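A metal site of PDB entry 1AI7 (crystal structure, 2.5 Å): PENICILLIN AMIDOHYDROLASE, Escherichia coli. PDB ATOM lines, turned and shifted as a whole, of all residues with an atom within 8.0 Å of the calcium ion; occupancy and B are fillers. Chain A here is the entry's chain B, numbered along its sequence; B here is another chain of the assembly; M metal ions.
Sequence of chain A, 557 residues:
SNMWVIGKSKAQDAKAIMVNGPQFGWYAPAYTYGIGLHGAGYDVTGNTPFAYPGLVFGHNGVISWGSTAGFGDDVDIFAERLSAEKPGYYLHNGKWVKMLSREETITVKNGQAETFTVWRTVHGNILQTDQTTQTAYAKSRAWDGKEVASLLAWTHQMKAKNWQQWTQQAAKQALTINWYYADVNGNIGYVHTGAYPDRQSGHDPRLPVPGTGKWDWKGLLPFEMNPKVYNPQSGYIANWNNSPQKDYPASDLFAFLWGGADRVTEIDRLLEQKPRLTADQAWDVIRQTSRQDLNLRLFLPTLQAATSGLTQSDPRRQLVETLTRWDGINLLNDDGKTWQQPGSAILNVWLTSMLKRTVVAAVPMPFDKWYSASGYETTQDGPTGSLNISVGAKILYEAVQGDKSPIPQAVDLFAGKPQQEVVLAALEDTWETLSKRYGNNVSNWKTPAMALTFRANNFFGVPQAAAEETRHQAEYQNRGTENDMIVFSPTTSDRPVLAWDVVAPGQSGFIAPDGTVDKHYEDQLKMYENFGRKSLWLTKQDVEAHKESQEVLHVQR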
ATOM      1  N   GLY A  72      12.293 -23.461  19.468  1.00  0.00           N
ATOM      2  CA  GLY A  72      11.577 -23.918  20.672  1.00  0.00           C
ATOM      3  C   GLY A  72      11.281 -22.645  21.451  1.00  0.00           C
ATOM      4  O   GLY A  72      11.789 -21.598  21.054  1.00  0.00           O
ATOM      5  N   ASP A  73      10.528 -22.711  22.522  1.00  0.00           N
ATOM      6  CA  ASP A  73      10.248 -21.540  23.337  1.00  0.00           C
ATOM      7  C   ASP A  73      11.211 -21.563  24.546  1.00  0.00           C
ATOM      8  O   ASP A  73      11.028 -22.293  25.539  1.00  0.00           O
ATOM      9  CB  ASP A  73       8.782 -21.488  23.803  1.00  0.00           C
ATOM     10  CG  ASP A  73       8.460 -20.325  24.676  1.00  0.00           C
ATOM     11  OD1 ASP A  73       9.380 -19.583  25.087  1.00  0.00           O
ATOM     12  OD2 ASP A  73       7.350 -19.874  25.043  1.00  0.00           O
ATOM     13  N   ASP A  74      12.255 -20.700  24.411  1.00  0.00           N
ATOM     14  CA  ASP A  74      13.259 -20.664  25.469  1.00  0.00           C
ATOM     15  C   ASP A  74      13.397 -19.278  26.062  1.00  0.00           C
ATOM     16  O   ASP A  74      14.466 -18.965  26.589  1.00  0.00           O
ATOM     17  CB  ASP A  74      14.612 -21.114  24.942  1.00  0.00           C
ATOM     18  CG  ASP A  74      15.136 -20.324  23.779  1.00  0.00           C
ATOM     19  OD1 ASP A  74      14.559 -19.290  23.367  1.00  0.00           O
ATOM     20  OD2 ASP A  74      16.164 -20.609  23.159  1.00  0.00           O
ATOM     21  N   VAL A  75      12.472 -18.401  25.744  1.00  0.00           N
ATOM     22  CA  VAL A  75      12.464 -17.042  26.256  1.00  0.00           C
ATOM     23  C   VAL A  75      11.068 -16.740  26.822  1.00  0.00           C
ATOM     24  O   VAL A  75      10.147 -16.949  26.024  1.00  0.00           O
ATOM     25  CB  VAL A  75      12.700 -16.051  25.124  1.00  0.00           C
ATOM     26  CG1 VAL A  75      12.608 -14.614  25.556  1.00  0.00           C
ATOM     27  CG2 VAL A  75      14.000 -16.245  24.364  1.00  0.00           C
ATOM     28  N   ASP A  76      10.927 -16.208  28.032  1.00  0.00           N
ATOM     29  CA  ASP A  76       9.640 -15.863  28.612  1.00  0.00           C
ATOM     30  C   ASP A  76       9.847 -14.466  29.205  1.00  0.00           C
ATOM     31  O   ASP A  76      10.982 -14.064  29.461  1.00  0.00           O
ATOM     32  CB  ASP A  76       9.045 -16.755  29.705  1.00  0.00           C
ATOM     33  CG  ASP A  76       8.844 -18.195  29.436  1.00  0.00           C
ATOM     34  OD1 ASP A  76       8.637 -18.638  28.263  1.00  0.00           O
ATOM     35  OD2 ASP A  76       8.861 -19.068  30.344  1.00  0.00           O
ATOM     36  N   ILE A  77       8.798 -13.708  29.393  1.00  0.00           N
ATOM     37  CA  ILE A  77       8.869 -12.307  29.803  1.00  0.00           C
ATOM     38  C   ILE A  77       8.290 -12.199  31.217  1.00  0.00           C
ATOM     39  O   ILE A  77       7.211 -12.725  31.505  1.00  0.00           O
ATOM     40  CB  ILE A  77       8.001 -11.436  28.870  1.00  0.00           C
ATOM     41  CG1 ILE A  77       8.402 -11.456  27.403  1.00  0.00           C
ATOM     42  CG2 ILE A  77       7.903 -10.002  29.391  1.00  0.00           C
ATOM     43  CD1 ILE A  77       9.783 -10.891  27.168  1.00  0.00           C
ATOM     44  N   SER A 140      13.666 -12.982  29.820  1.00  0.00           N
ATOM     45  CA  SER A 140      14.430 -14.022  30.434  1.00  0.00           C
ATOM     46  C   SER A 140      14.716 -15.136  29.456  1.00  0.00           C
ATOM     47  O   SER A 140      13.812 -15.747  28.901  1.00  0.00           O
ATOM     48  CB  SER A 140      13.694 -14.395  31.703  1.00  0.00           C
ATOM     49  OG  SER A 140      14.028 -15.676  32.122  1.00  0.00           O
ATOM     50  N   PRO A 197      13.436 -24.010  30.033  1.00  0.00           N
ATOM     51  CA  PRO A 197      13.033 -23.787  31.396  1.00  0.00           C
ATOM     52  C   PRO A 197      12.143 -24.859  31.993  1.00  0.00           C
ATOM     53  O   PRO A 197      11.415 -25.548  31.294  1.00  0.00           O
ATOM     54  CB  PRO A 197      12.233 -22.447  31.434  1.00  0.00           C
ATOM     55  CG  PRO A 197      11.774 -22.358  30.004  1.00  0.00           C
ATOM     56  CD  PRO A 197      12.765 -23.071  29.113  1.00  0.00           C
ATOM     57  N   ARG A 199       9.183 -25.027  33.978  1.00  0.00           N
ATOM     58  CA  ARG A 199       8.244 -23.999  34.444  1.00  0.00           C
ATOM     59  C   ARG A 199       7.332 -24.534  35.549  1.00  0.00           C
ATOM     60  O   ARG A 199       6.994 -25.724  35.611  1.00  0.00           O
ATOM     61  CB  ARG A 199       7.433 -23.510  33.231  1.00  0.00           C
ATOM     62  CG  ARG A 199       8.256 -22.904  32.099  1.00  0.00           C
ATOM     63  CD  ARG A 199       7.379 -22.356  30.977  1.00  0.00           C
ATOM     64  NE  ARG A 199       8.029 -21.546  29.964  1.00  0.00           N
ATOM     65  CZ  ARG A 199       8.523 -22.138  28.854  1.00  0.00           C
ATOM     66  NH1 ARG A 199       8.451 -23.437  28.676  1.00  0.00           N
ATOM     67  NH2 ARG A 199       9.107 -21.366  27.961  1.00  0.00           N
ATOM     68  N   HIS A 203       1.788 -22.177  34.276  1.00  0.00           N
ATOM     69  CA  HIS A 203       2.464 -21.149  33.529  1.00  0.00           C
ATOM     70  C   HIS A 203       2.160 -21.335  32.041  1.00  0.00           C
ATOM     71  O   HIS A 203       2.551 -22.382  31.510  1.00  0.00           O
ATOM     72  CB  HIS A 203       3.980 -21.343  33.708  1.00  0.00           C
ATOM     73  CG  HIS A 203       4.820 -20.320  33.035  1.00  0.00           C
ATOM     74  ND1 HIS A 203       6.013 -19.879  33.578  1.00  0.00           N
ATOM     75  CD2 HIS A 203       4.682 -19.600  31.904  1.00  0.00           C
ATOM     76  CE1 HIS A 203       6.587 -18.941  32.840  1.00  0.00           C
ATOM     77  NE2 HIS A 203       5.757 -18.751  31.823  1.00  0.00           N
ATOM     78  N   ASP A 204       1.420 -20.453  31.399  1.00  0.00           N
ATOM     79  CA  ASP A 204       1.150 -20.578  29.957  1.00  0.00           C
ATOM     80  C   ASP A 204       2.306 -19.853  29.246  1.00  0.00           C
ATOM     81  O   ASP A 204       2.519 -18.637  29.459  1.00  0.00           O
ATOM     82  CB  ASP A 204      -0.168 -19.845  29.695  1.00  0.00           C
ATOM     83  CG  ASP A 204      -0.604 -19.860  28.237  1.00  0.00           C
ATOM     84  OD1 ASP A 204       0.193 -19.992  27.271  1.00  0.00           O
ATOM     85  OD2 ASP A 204      -1.839 -19.774  28.028  1.00  0.00           O
ATOM     86  N   PRO A 205       3.151 -20.537  28.501  1.00  0.00           N
ATOM     87  CA  PRO A 205       4.401 -19.965  27.995  1.00  0.00           C
ATOM     88  C   PRO A 205       4.257 -18.957  26.884  1.00  0.00           C
ATOM     89  O   PRO A 205       5.207 -18.285  26.479  1.00  0.00           O
ATOM     90  CB  PRO A 205       5.312 -21.136  27.585  1.00  0.00           C
ATOM     91  CG  PRO A 205       4.333 -22.248  27.494  1.00  0.00           C
ATOM     92  CD  PRO A 205       3.058 -21.983  28.299  1.00  0.00           C
ATOM     93  N   ARG A 206       3.046 -18.657  26.412  1.00  0.00           N
ATOM     94  CA  ARG A 206       2.756 -17.731  25.355  1.00  0.00           C
ATOM     95  C   ARG A 206       2.493 -16.339  25.871  1.00  0.00           C
ATOM     96  O   ARG A 206       2.312 -15.473  25.014  1.00  0.00           O
ATOM     97  CB  ARG A 206       1.492 -18.085  24.574  1.00  0.00           C
ATOM     98  CG  ARG A 206       1.500 -19.440  23.886  1.00  0.00           C
ATOM     99  CD  ARG A 206       0.136 -19.982  23.544  1.00  0.00           C
ATOM    100  NE  ARG A 206      -0.843 -20.021  24.608  1.00  0.00           N
ATOM    101  CZ  ARG A 206      -2.065 -20.552  24.540  1.00  0.00           C
ATOM    102  NH1 ARG A 206      -2.461 -21.078  23.379  1.00  0.00           N
ATOM    103  NH2 ARG A 206      -2.873 -20.545  25.596  1.00  0.00           N
ATOM    104  N   LEU A 207       2.427 -16.171  27.176  1.00  0.00           N
ATOM    105  CA  LEU A 207       2.054 -14.860  27.741  1.00  0.00           C
ATOM    106  C   LEU A 207       2.922 -14.534  28.932  1.00  0.00           C
ATOM    107  O   LEU A 207       3.364 -15.426  29.657  1.00  0.00           O
ATOM    108  CB  LEU A 207       0.584 -15.020  28.213  1.00  0.00           C
ATOM    109  CG  LEU A 207      -0.464 -15.290  27.100  1.00  0.00           C
ATOM    110  CD1 LEU A 207      -1.653 -16.087  27.586  1.00  0.00           C
ATOM    111  CD2 LEU A 207      -0.824 -13.932  26.515  1.00  0.00           C
ATOM    112  N   PRO A 208       3.081 -13.293  29.315  1.00  0.00           N
ATOM    113  CA  PRO A 208       3.907 -12.875  30.419  1.00  0.00           C
ATOM    114  C   PRO A 208       3.553 -13.460  31.765  1.00  0.00           C
ATOM    115  O   PRO A 208       2.423 -13.840  31.954  1.00  0.00           O
ATOM    116  CB  PRO A 208       3.798 -11.324  30.501  1.00  0.00           C
ATOM    117  CG  PRO A 208       3.309 -10.981  29.118  1.00  0.00           C
ATOM    118  CD  PRO A 208       2.598 -12.172  28.505  1.00  0.00           C
ATOM    119  N   TRP A 217      11.000 -19.674  37.188  1.00  0.00           N
ATOM    120  CA  TRP A 217      11.314 -21.020  36.714  1.00  0.00           C
ATOM    121  C   TRP A 217      11.934 -21.807  37.871  1.00  0.00           C
ATOM    122  O   TRP A 217      12.530 -21.241  38.786  1.00  0.00           O
ATOM    123  CB  TRP A 217      12.345 -20.946  35.605  1.00  0.00           C
ATOM    124  CG  TRP A 217      11.945 -20.242  34.350  1.00  0.00           C
ATOM    125  CD1 TRP A 217      10.685 -20.045  33.878  1.00  0.00           C
ATOM    126  CD2 TRP A 217      12.834 -19.741  33.348  1.00  0.00           C
ATOM    127  NE1 TRP A 217      10.745 -19.404  32.673  1.00  0.00           N
ATOM    128  CE2 TRP A 217      12.037 -19.200  32.309  1.00  0.00           C
ATOM    129  CE3 TRP A 217      14.237 -19.708  33.226  1.00  0.00           C
ATOM    130  CZ2 TRP A 217      12.564 -18.623  31.164  1.00  0.00           C
ATOM    131  CZ3 TRP A 217      14.764 -19.083  32.105  1.00  0.00           C
ATOM    132  CH2 TRP A 217      13.943 -18.570  31.069  1.00  0.00           C
ATOM    133  N   ALA A 250       6.124 -24.798  20.276  1.00  0.00           N
ATOM    134  CA  ALA A 250       6.932 -23.998  19.406  1.00  0.00           C
ATOM    135  C   ALA A 250       7.114 -22.662  20.116  1.00  0.00           C
ATOM    136  O   ALA A 250       6.454 -22.443  21.127  1.00  0.00           O
ATOM    137  CB  ALA A 250       6.257 -23.650  18.089  1.00  0.00           C
ATOM    138  N   SER A 251       8.020 -21.892  19.542  1.00  0.00           N
ATOM    139  CA  SER A 251       8.267 -20.520  19.982  1.00  0.00           C
ATOM    140  C   SER A 251       6.930 -19.889  20.331  1.00  0.00           C
ATOM    141  O   SER A 251       6.005 -20.117  19.558  1.00  0.00           O
ATOM    142  CB  SER A 251       8.721 -19.789  18.719  1.00  0.00           C
ATOM    143  OG  SER A 251       8.930 -18.402  19.017  1.00  0.00           O
ATOM    144  N   ASP A 252       6.869 -18.844  21.134  1.00  0.00           N
ATOM    145  CA  ASP A 252       5.628 -18.146  21.407  1.00  0.00           C
ATOM    146  C   ASP A 252       5.313 -17.051  20.405  1.00  0.00           C
ATOM    147  O   ASP A 252       4.273 -16.350  20.512  1.00  0.00           O
ATOM    148  CB  ASP A 252       5.615 -17.611  22.839  1.00  0.00           C
ATOM    149  CG  ASP A 252       6.670 -16.576  23.132  1.00  0.00           C
ATOM    150  OD1 ASP A 252       6.824 -15.605  22.349  1.00  0.00           O
ATOM    151  OD2 ASP A 252       7.431 -16.638  24.151  1.00  0.00           O
ATOM    152  N   LEU A 253       6.123 -16.881  19.364  1.00  0.00           N
ATOM    153  CA  LEU A 253       5.880 -15.887  18.328  1.00  0.00           C
ATOM    154  C   LEU A 253       4.484 -16.020  17.694  1.00  0.00           C
ATOM    155  O   LEU A 253       4.190 -17.124  17.153  1.00  0.00           O
ATOM    156  CB  LEU A 253       6.865 -16.030  17.168  1.00  0.00           C
ATOM    157  CG  LEU A 253       8.250 -15.489  17.430  1.00  0.00           C
ATOM    158  CD1 LEU A 253       9.175 -15.904  16.294  1.00  0.00           C
ATOM    159  CD2 LEU A 253       8.241 -13.983  17.670  1.00  0.00           C
ATOM    160  N   SER B 149      13.730 -15.198  20.183  1.00  0.00           N
ATOM    161  CA  SER B 149      12.440 -14.745  19.699  1.00  0.00           C
ATOM    162  C   SER B 149      11.320 -14.799  20.740  1.00  0.00           C
ATOM    163  O   SER B 149      11.168 -15.884  21.321  1.00  0.00           O
ATOM    164  CB  SER B 149      12.006 -15.688  18.580  1.00  0.00           C
ATOM    165  OG  SER B 149      12.871 -15.598  17.502  1.00  0.00           O
ATOM    166  N   THR B 150      10.527 -13.748  20.892  1.00  0.00           N
ATOM    167  CA  THR B 150       9.380 -13.859  21.800  1.00  0.00           C
ATOM    168  C   THR B 150       8.405 -12.790  21.313  1.00  0.00           C
ATOM    169  O   THR B 150       8.877 -11.736  20.915  1.00  0.00           O
ATOM    170  CB  THR B 150       9.684 -13.673  23.288  1.00  0.00           C
ATOM    171  OG1 THR B 150       8.533 -13.954  24.099  1.00  0.00           O
ATOM    172  CG2 THR B 150       9.997 -12.221  23.656  1.00  0.00           C
ATOM    173  N   SER B 151       7.105 -12.939  21.514  1.00  0.00           N
ATOM    174  CA  SER B 151       6.172 -11.859  21.213  1.00  0.00           C
ATOM    175  C   SER B 151       5.141 -11.885  22.345  1.00  0.00           C
ATOM    176  O   SER B 151       4.048 -11.366  22.065  1.00  0.00           O
ATOM    177  CB  SER B 151       5.489 -11.944  19.823  1.00  0.00           C
ATOM    178  OG  SER B 151       4.718 -13.157  19.782  1.00  0.00           O
ATOM    179  N   GLU B 152       5.601 -12.274  23.548  1.00  0.00           N
ATOM    180  CA  GLU B 152       4.671 -12.449  24.663  1.00  0.00           C
ATOM    181  C   GLU B 152       3.884 -11.196  25.008  1.00  0.00           C
ATOM    182  O   GLU B 152       2.684 -11.243  25.320  1.00  0.00           O
ATOM    183  CB  GLU B 152       5.303 -13.028  25.942  1.00  0.00           C
ATOM    184  CG  GLU B 152       5.596 -14.518  25.897  1.00  0.00           C
ATOM    185  CD  GLU B 152       6.293 -15.011  27.155  1.00  0.00           C
ATOM    186  OE1 GLU B 152       6.223 -14.240  28.153  1.00  0.00           O
ATOM    187  OE2 GLU B 152       6.861 -16.139  27.090  1.00  0.00           O
ATOM    188  N   ASN B 155       1.311 -10.846  22.254  1.00  0.00           N
ATOM    189  CA  ASN B 155       0.316 -11.891  22.510  1.00  0.00           C
ATOM    190  C   ASN B 155      -0.746 -11.419  23.462  1.00  0.00           C
ATOM    191  O   ASN B 155      -1.968 -11.616  23.222  1.00  0.00           O
ATOM    192  CB  ASN B 155       1.001 -13.171  23.021  1.00  0.00           C
ATOM    193  CG  ASN B 155       1.830 -13.709  21.869  1.00  0.00           C
ATOM    194  OD1 ASN B 155       2.335 -14.791  22.135  1.00  0.00           O
ATOM    195  ND2 ASN B 155       2.001 -13.094  20.692  1.00  0.00           N
HETATM  196 CA    CA M   1       7.641 -17.880  26.028  1.00  0.00          CA
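Of the 25 residues printed, 6 come within 4 Å of the calcium ion.
OE1 of Glu 152 of chain B is in hydrogen-bond range of N of Ile 77 (2.9 Å). O of Asp 73 sits at hydrogen-bond distance from NH2 of Arg 199 (3.2 Å). OD1 of Asp 252 is in hydrogen-bond range of N of Ser 151 of chain B. The backbone carbonyl oxygen (O) of Asp 252 lies close to the side-chain amide oxygen (OD1) of Asn 155 of chain B, at 3.0 Å. NE of Arg 199 lies within salt-bridge range of OD2 of Asp 76 (2.6 Å). OD2 of Asp 76 sits close to NE2 of His 203 (3.5 Å). N of Ser 140 lies within hydrogen-bond range of O of Asp 76 (2.9 Å). OD2 of Asp 76 sits at hydrogen-bond distance from NE1 of Trp 217 (3.0 Å).
The calcium ion is bound by OE2 of Glu 152 of chain B (2.2 Å), OD2 of Asp 73 (2.2 Å), OD2 of Asp 252 (2.3 Å), O of Pro 205 (2.5 Å), OD1 of Asp 76 (2.6 Å), OD1 of Asp 73 (2.6 Å) and O of Val 75 (2.7 Å). The calcium ion has seven donor atoms within binding distance.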
